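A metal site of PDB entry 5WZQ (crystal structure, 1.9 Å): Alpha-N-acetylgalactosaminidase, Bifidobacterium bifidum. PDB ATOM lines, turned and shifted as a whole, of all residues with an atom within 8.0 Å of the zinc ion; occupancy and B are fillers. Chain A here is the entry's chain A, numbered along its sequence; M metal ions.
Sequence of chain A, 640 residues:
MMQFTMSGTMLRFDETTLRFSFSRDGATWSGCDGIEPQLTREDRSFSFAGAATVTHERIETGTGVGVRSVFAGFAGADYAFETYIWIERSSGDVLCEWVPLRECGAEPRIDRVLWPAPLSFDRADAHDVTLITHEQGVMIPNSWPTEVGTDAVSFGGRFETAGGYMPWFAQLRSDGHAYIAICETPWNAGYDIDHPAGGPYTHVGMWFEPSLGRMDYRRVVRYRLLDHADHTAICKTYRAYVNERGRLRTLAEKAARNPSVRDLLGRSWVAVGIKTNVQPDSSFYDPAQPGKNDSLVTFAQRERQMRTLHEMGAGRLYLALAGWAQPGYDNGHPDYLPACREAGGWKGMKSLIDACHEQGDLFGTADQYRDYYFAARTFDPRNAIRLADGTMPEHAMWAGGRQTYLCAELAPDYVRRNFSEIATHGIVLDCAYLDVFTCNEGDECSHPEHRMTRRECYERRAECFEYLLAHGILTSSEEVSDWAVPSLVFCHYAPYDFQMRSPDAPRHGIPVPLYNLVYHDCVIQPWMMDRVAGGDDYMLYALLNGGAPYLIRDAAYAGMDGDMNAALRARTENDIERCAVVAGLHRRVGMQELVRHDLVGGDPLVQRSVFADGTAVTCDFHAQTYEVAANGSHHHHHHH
The zinc ion is bound by ND1 of His 450 (2.0 Å), O of His 450 (2.0 Å), SG of Cys 445 (2.2 Å) and SG of Cys 407 (2.3 Å).
Three residues have an atom within 4 Å of the zinc ion: Cys 407, Cys 445 and His 450.
The nearest printed residue that does not touch the zinc ion is His 447 (4.1 Å).
The side-chain sulfur (SG) of Cys 445 sits close to the backbone NH (N) of His 447 (3.3 Å).
The backbone carbonyl oxygen (O) of Asn 383 sits at hydrogen-bond distance from the backbone NH (N) of Cys 407 (3.1 Å).
N of Met 452 is in hydrogen-bond range of O of Cys 445, 2.7 Å away.
SG of Cys 407 lies close to N of Glu 409 (3.7 Å).
A ring nitrogen (NE2) of His 450 lies within hydrogen-bond range of the backbone carbonyl oxygen of Arg 382 (2.7 Å).
N of Arg 386 sits close to SG of Cys 445 (3.6 Å).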
ATOM      1  N   ARG A 382       9.538 -28.125   0.427  1.00  0.00           N
ATOM      2  CA  ARG A 382       8.718 -27.276   1.245  1.00  0.00           C
ATOM      3  C   ARG A 382       9.523 -26.094   1.815  1.00  0.00           C
ATOM      4  O   ARG A 382       8.946 -25.145   2.280  1.00  0.00           O
ATOM      5  CB  ARG A 382       8.076 -28.052   2.416  1.00  0.00           C
ATOM      6  CG  ARG A 382       9.031 -28.342   3.567  1.00  0.00           C
ATOM      7  CD  ARG A 382       8.427 -29.227   4.649  1.00  0.00           C
ATOM      8  NE  ARG A 382       7.084 -28.757   5.051  1.00  0.00           N
ATOM      9  CZ  ARG A 382       6.107 -29.592   5.403  1.00  0.00           C
ATOM     10  NH1 ARG A 382       6.336 -30.889   5.447  1.00  0.00           N
ATOM     11  NH2 ARG A 382       4.927 -29.132   5.736  1.00  0.00           N
ATOM     12  N   ASN A 383      10.858 -26.184   1.807  1.00  0.00           N
ATOM     13  CA  ASN A 383      11.665 -25.048   2.294  1.00  0.00           C
ATOM     14  C   ASN A 383      11.947 -24.055   1.188  1.00  0.00           C
ATOM     15  O   ASN A 383      12.569 -22.991   1.406  1.00  0.00           O
ATOM     16  CB  ASN A 383      13.024 -25.561   2.844  1.00  0.00           C
ATOM     17  CG  ASN A 383      12.899 -26.502   4.040  1.00  0.00           C
ATOM     18  OD1 ASN A 383      12.101 -26.290   4.931  1.00  0.00           O
ATOM     19  ND2 ASN A 383      13.728 -27.606   4.037  1.00  0.00           N
ATOM     20  N   ALA A 384      11.600 -24.418  -0.018  1.00  0.00           N
ATOM     21  CA  ALA A 384      11.975 -23.609  -1.160  1.00  0.00           C
ATOM     22  C   ALA A 384      10.953 -22.532  -1.443  1.00  0.00           C
ATOM     23  O   ALA A 384       9.784 -22.661  -1.092  1.00  0.00           O
ATOM     24  CB  ALA A 384      12.145 -24.476  -2.396  1.00  0.00           C
ATOM     25  N   ILE A 385      11.431 -21.552  -2.188  1.00  0.00           N
ATOM     26  CA  ILE A 385      10.652 -20.463  -2.755  1.00  0.00           C
ATOM     27  C   ILE A 385       9.537 -21.015  -3.603  1.00  0.00           C
ATOM     28  O   ILE A 385       9.692 -22.045  -4.246  1.00  0.00           O
ATOM     29  CB  ILE A 385      11.615 -19.612  -3.616  1.00  0.00           C
ATOM     30  CG1 ILE A 385      12.471 -18.729  -2.701  1.00  0.00           C
ATOM     31  CG2 ILE A 385      10.904 -18.683  -4.614  1.00  0.00           C
ATOM     32  CD1 ILE A 385      11.724 -17.551  -2.111  1.00  0.00           C
ATOM     33  N   ARG A 386       8.383 -20.326  -3.567  1.00  0.00           N
ATOM     34  CA  ARG A 386       7.394 -20.392  -4.641  1.00  0.00           C
ATOM     35  C   ARG A 386       7.175 -18.982  -5.154  1.00  0.00           C
ATOM     36  O   ARG A 386       6.998 -18.045  -4.407  1.00  0.00           O
ATOM     37  CB  ARG A 386       6.051 -20.910  -4.117  1.00  0.00           C
ATOM     38  CG  ARG A 386       6.069 -22.341  -3.551  1.00  0.00           C
ATOM     39  CD  ARG A 386       6.614 -23.394  -4.582  1.00  0.00           C
ATOM     40  NE  ARG A 386       6.493 -24.729  -3.979  1.00  0.00           N
ATOM     41  CZ  ARG A 386       7.391 -25.283  -3.179  1.00  0.00           C
ATOM     42  NH1 ARG A 386       8.526 -24.641  -2.898  1.00  0.00           N
ATOM     43  NH2 ARG A 386       7.164 -26.524  -2.671  1.00  0.00           N
ATOM     44  N   TYR A 405      15.795 -22.196  -4.878  1.00  0.00           N
ATOM     45  CA  TYR A 405      16.259 -21.235  -3.885  1.00  0.00           C
ATOM     46  C   TYR A 405      15.643 -21.533  -2.516  1.00  0.00           C
ATOM     47  O   TYR A 405      14.449 -21.860  -2.410  1.00  0.00           O
ATOM     48  CB  TYR A 405      15.920 -19.823  -4.303  1.00  0.00           C
ATOM     49  CG  TYR A 405      16.462 -19.479  -5.648  1.00  0.00           C
ATOM     50  CD1 TYR A 405      17.850 -19.478  -5.877  1.00  0.00           C
ATOM     51  CD2 TYR A 405      15.587 -19.169  -6.707  1.00  0.00           C
ATOM     52  CE1 TYR A 405      18.373 -19.181  -7.127  1.00  0.00           C
ATOM     53  CE2 TYR A 405      16.073 -18.856  -7.969  1.00  0.00           C
ATOM     54  CZ  TYR A 405      17.472 -18.870  -8.175  1.00  0.00           C
ATOM     55  OH  TYR A 405      17.945 -18.608  -9.399  1.00  0.00           O
ATOM     56  N   LEU A 406      16.466 -21.465  -1.479  1.00  0.00           N
ATOM     57  CA  LEU A 406      15.978 -21.554  -0.083  1.00  0.00           C
ATOM     58  C   LEU A 406      15.244 -20.232   0.250  1.00  0.00           C
ATOM     59  O   LEU A 406      15.799 -19.171   0.049  1.00  0.00           O
ATOM     60  CB  LEU A 406      17.164 -21.735   0.841  1.00  0.00           C
ATOM     61  CG  LEU A 406      16.816 -21.881   2.341  1.00  0.00           C
ATOM     62  CD1 LEU A 406      16.048 -23.179   2.651  1.00  0.00           C
ATOM     63  CD2 LEU A 406      18.096 -21.803   3.185  1.00  0.00           C
ATOM     64  N   CYS A 407      14.020 -20.302   0.820  1.00  0.00           N
ATOM     65  CA  CYS A 407      13.305 -19.101   1.142  1.00  0.00           C
ATOM     66  C   CYS A 407      14.067 -18.403   2.273  1.00  0.00           C
ATOM     67  O   CYS A 407      14.402 -19.041   3.251  1.00  0.00           O
ATOM     68  CB  CYS A 407      11.870 -19.417   1.622  1.00  0.00           C
ATOM     69  SG  CYS A 407      11.033 -17.904   2.089  1.00  0.00           S
ATOM     70  N   ALA A 408      14.342 -17.099   2.142  1.00  0.00           N
ATOM     71  CA  ALA A 408      15.192 -16.422   3.091  1.00  0.00           C
ATOM     72  C   ALA A 408      14.585 -16.358   4.501  1.00  0.00           C
ATOM     73  O   ALA A 408      15.338 -16.177   5.452  1.00  0.00           O
ATOM     74  CB  ALA A 408      15.533 -15.002   2.596  1.00  0.00           C
ATOM     75  N   GLU A 409      13.263 -16.537   4.635  1.00  0.00           N
ATOM     76  CA  GLU A 409      12.639 -16.642   5.955  1.00  0.00           C
ATOM     77  C   GLU A 409      13.326 -17.714   6.833  1.00  0.00           C
ATOM     78  O   GLU A 409      13.296 -17.648   8.043  1.00  0.00           O
ATOM     79  CB  GLU A 409      11.185 -17.058   5.764  1.00  0.00           C
ATOM     80  CG  GLU A 409      10.267 -15.982   5.163  1.00  0.00           C
ATOM     81  CD  GLU A 409      10.002 -14.846   6.144  1.00  0.00           C
ATOM     82  OE1 GLU A 409       9.344 -15.102   7.151  1.00  0.00           O
ATOM     83  OE2 GLU A 409      10.497 -13.724   5.933  1.00  0.00           O
ATOM     84  N   LEU A 410      13.898 -18.725   6.151  1.00  0.00           N
ATOM     85  CA  LEU A 410      14.535 -19.863   6.764  1.00  0.00           C
ATOM     86  C   LEU A 410      16.072 -19.774   6.793  1.00  0.00           C
ATOM     87  O   LEU A 410      16.725 -20.594   7.480  1.00  0.00           O
ATOM     88  CB  LEU A 410      14.061 -21.169   6.050  1.00  0.00           C
ATOM     89  CG  LEU A 410      12.530 -21.358   5.915  1.00  0.00           C
ATOM     90  CD1 LEU A 410      12.247 -22.718   5.244  1.00  0.00           C
ATOM     91  CD2 LEU A 410      11.832 -21.337   7.262  1.00  0.00           C
ATOM     92  N   ASP A 443      14.417 -12.411  -3.265  1.00  0.00           N
ATOM     93  CA  ASP A 443      13.321 -13.205  -3.767  1.00  0.00           C
ATOM     94  C   ASP A 443      12.023 -12.845  -3.048  1.00  0.00           C
ATOM     95  O   ASP A 443      12.019 -12.302  -1.909  1.00  0.00           O
ATOM     96  CB  ASP A 443      13.582 -14.660  -3.418  1.00  0.00           C
ATOM     97  CG  ASP A 443      14.841 -15.171  -4.038  1.00  0.00           C
ATOM     98  OD1 ASP A 443      15.007 -14.986  -5.288  1.00  0.00           O
ATOM     99  OD2 ASP A 443      15.649 -15.802  -3.299  1.00  0.00           O
ATOM    100  N   GLU A 444      10.917 -13.125  -3.734  1.00  0.00           N
ATOM    101  CA  GLU A 444       9.632 -13.104  -3.076  1.00  0.00           C
ATOM    102  C   GLU A 444       9.108 -14.520  -3.083  1.00  0.00           C
ATOM    103  O   GLU A 444       9.557 -15.348  -3.897  1.00  0.00           O
ATOM    104  CB  GLU A 444       8.691 -12.065  -3.692  1.00  0.00           C
ATOM    105  CG  GLU A 444       8.298 -12.419  -5.152  1.00  0.00           C
ATOM    106  CD  GLU A 444       7.229 -11.480  -5.659  1.00  0.00           C
ATOM    107  OE1 GLU A 444       7.107 -10.338  -5.162  1.00  0.00           O
ATOM    108  OE2 GLU A 444       6.480 -11.931  -6.570  1.00  0.00           O
ATOM    109  N   CYS A 445       8.271 -14.837  -2.111  1.00  0.00           N
ATOM    110  CA  CYS A 445       7.771 -16.183  -1.878  1.00  0.00           C
ATOM    111  C   CYS A 445       6.296 -16.147  -1.482  1.00  0.00           C
ATOM    112  O   CYS A 445       5.918 -15.503  -0.515  1.00  0.00           O
ATOM    113  CB  CYS A 445       8.518 -16.810  -0.711  1.00  0.00           C
ATOM    114  SG  CYS A 445       8.201 -18.575  -0.440  1.00  0.00           S
ATOM    115  N   SER A 446       5.518 -16.982  -2.157  1.00  0.00           N
ATOM    116  CA  SER A 446       4.061 -17.060  -1.908  1.00  0.00           C
ATOM    117  C   SER A 446       3.857 -18.363  -1.130  1.00  0.00           C
ATOM    118  O   SER A 446       2.703 -18.749  -0.903  1.00  0.00           O
ATOM    119  CB  SER A 446       3.326 -17.125  -3.278  1.00  0.00           C
ATOM    120  OG  SER A 446       3.673 -18.316  -4.013  1.00  0.00           O
ATOM    121  N   HIS A 447       4.921 -19.060  -0.732  1.00  0.00           N
ATOM    122  CA  HIS A 447       4.692 -20.372  -0.077  1.00  0.00           C
ATOM    123  C   HIS A 447       3.982 -20.023   1.248  1.00  0.00           C
ATOM    124  O   HIS A 447       4.448 -19.179   1.971  1.00  0.00           O
ATOM    125  CB  HIS A 447       5.987 -21.146   0.178  1.00  0.00           C
ATOM    126  CG  HIS A 447       5.769 -22.573   0.586  1.00  0.00           C
ATOM    127  ND1 HIS A 447       4.959 -22.929   1.649  1.00  0.00           N
ATOM    128  CD2 HIS A 447       6.185 -23.732   0.019  1.00  0.00           C
ATOM    129  CE1 HIS A 447       4.945 -24.243   1.755  1.00  0.00           C
ATOM    130  NE2 HIS A 447       5.668 -24.760   0.763  1.00  0.00           N
ATOM    131  N   PRO A 448       2.793 -20.594   1.499  1.00  0.00           N
ATOM    132  CA  PRO A 448       2.045 -20.288   2.723  1.00  0.00           C
ATOM    133  C   PRO A 448       2.765 -20.545   4.056  1.00  0.00           C
ATOM    134  O   PRO A 448       2.443 -19.875   5.027  1.00  0.00           O
ATOM    135  CB  PRO A 448       0.783 -21.150   2.587  1.00  0.00           C
ATOM    136  CG  PRO A 448       0.708 -21.542   1.160  1.00  0.00           C
ATOM    137  CD  PRO A 448       2.088 -21.578   0.641  1.00  0.00           C
ATOM    138  N   GLU A 449       3.701 -21.513   4.117  1.00  0.00           N
ATOM    139  CA  GLU A 449       4.456 -21.760   5.325  1.00  0.00           C
ATOM    140  C   GLU A 449       5.545 -20.712   5.560  1.00  0.00           C
ATOM    141  O   GLU A 449       6.109 -20.624   6.691  1.00  0.00           O
ATOM    142  CB  GLU A 449       5.073 -23.182   5.364  1.00  0.00           C
ATOM    143  CG  GLU A 449       4.099 -24.326   5.089  1.00  0.00           C
ATOM    144  CD  GLU A 449       4.746 -25.709   4.923  1.00  0.00           C
ATOM    145  OE1 GLU A 449       5.980 -25.922   5.035  1.00  0.00           O
ATOM    146  OE2 GLU A 449       3.951 -26.661   4.653  1.00  0.00           O
ATOM    147  N   HIS A 450       5.866 -19.937   4.536  1.00  0.00           N
ATOM    148  CA  HIS A 450       6.841 -18.869   4.709  1.00  0.00           C
ATOM    149  C   HIS A 450       6.699 -17.821   3.629  1.00  0.00           C
ATOM    150  O   HIS A 450       7.529 -17.716   2.777  1.00  0.00           O
ATOM    151  CB  HIS A 450       8.295 -19.396   4.771  1.00  0.00           C
ATOM    152  CG  HIS A 450       8.529 -20.579   3.875  1.00  0.00           C
ATOM    153  ND1 HIS A 450       8.628 -20.461   2.509  1.00  0.00           N
ATOM    154  CD2 HIS A 450       8.638 -21.898   4.164  1.00  0.00           C
ATOM    155  CE1 HIS A 450       8.824 -21.666   1.989  1.00  0.00           C
ATOM    156  NE2 HIS A 450       8.836 -22.558   2.974  1.00  0.00           N
ATOM    157  N   ARG A 451       5.628 -17.042   3.660  1.00  0.00           N
ATOM    158  CA  ARG A 451       5.396 -16.045   2.639  1.00  0.00           C
ATOM    159  C   ARG A 451       6.368 -14.893   2.856  1.00  0.00           C
ATOM    160  O   ARG A 451       6.667 -14.495   3.991  1.00  0.00           O
ATOM    161  CB  ARG A 451       3.972 -15.571   2.812  1.00  0.00           C
ATOM    162  CG  ARG A 451       3.512 -14.667   1.732  1.00  0.00           C
ATOM    163  CD  ARG A 451       2.077 -14.233   1.999  1.00  0.00           C
ATOM    164  NE  ARG A 451       1.898 -13.587   3.299  1.00  0.00           N
ATOM    165  CZ  ARG A 451       2.231 -12.336   3.619  1.00  0.00           C
ATOM    166  NH1 ARG A 451       2.850 -11.546   2.736  1.00  0.00           N
ATOM    167  NH2 ARG A 451       1.961 -11.879   4.837  1.00  0.00           N
ATOM    168  N   MET A 452       6.901 -14.374   1.784  1.00  0.00           N
ATOM    169  CA  MET A 452       7.899 -13.383   1.922  1.00  0.00           C
ATOM    170  C   MET A 452       7.904 -12.325   0.806  1.00  0.00           C
ATOM    171  O   MET A 452       7.843 -12.669  -0.352  1.00  0.00           O
ATOM    172  CB  MET A 452       9.277 -14.090   2.002  1.00  0.00           C
ATOM    173  CG  MET A 452      10.460 -13.114   2.237  1.00  0.00           C
ATOM    174  SD  MET A 452      12.026 -14.014   2.284  1.00  0.00           S
ATOM    175  CE  MET A 452      12.070 -14.624   0.570  1.00  0.00           C
ATOM    176  N   THR A 453       7.978 -11.052   1.170  1.00  0.00           N
ATOM    177  CA  THR A 453       8.124 -10.035   0.142  1.00  0.00           C
ATOM    178  C   THR A 453       9.627  -9.817  -0.190  1.00  0.00           C
ATOM    179  O   THR A 453      10.481 -10.244   0.533  1.00  0.00           O
ATOM    180  CB  THR A 453       7.521  -8.705   0.523  1.00  0.00           C
ATOM    181  OG1 THR A 453       8.203  -8.183   1.665  1.00  0.00           O
ATOM    182  CG2 THR A 453       6.017  -8.837   0.771  1.00  0.00           C
HETATM  183 ZN    ZN M   1       8.901 -18.687   1.650  1.00  0.00          ZN
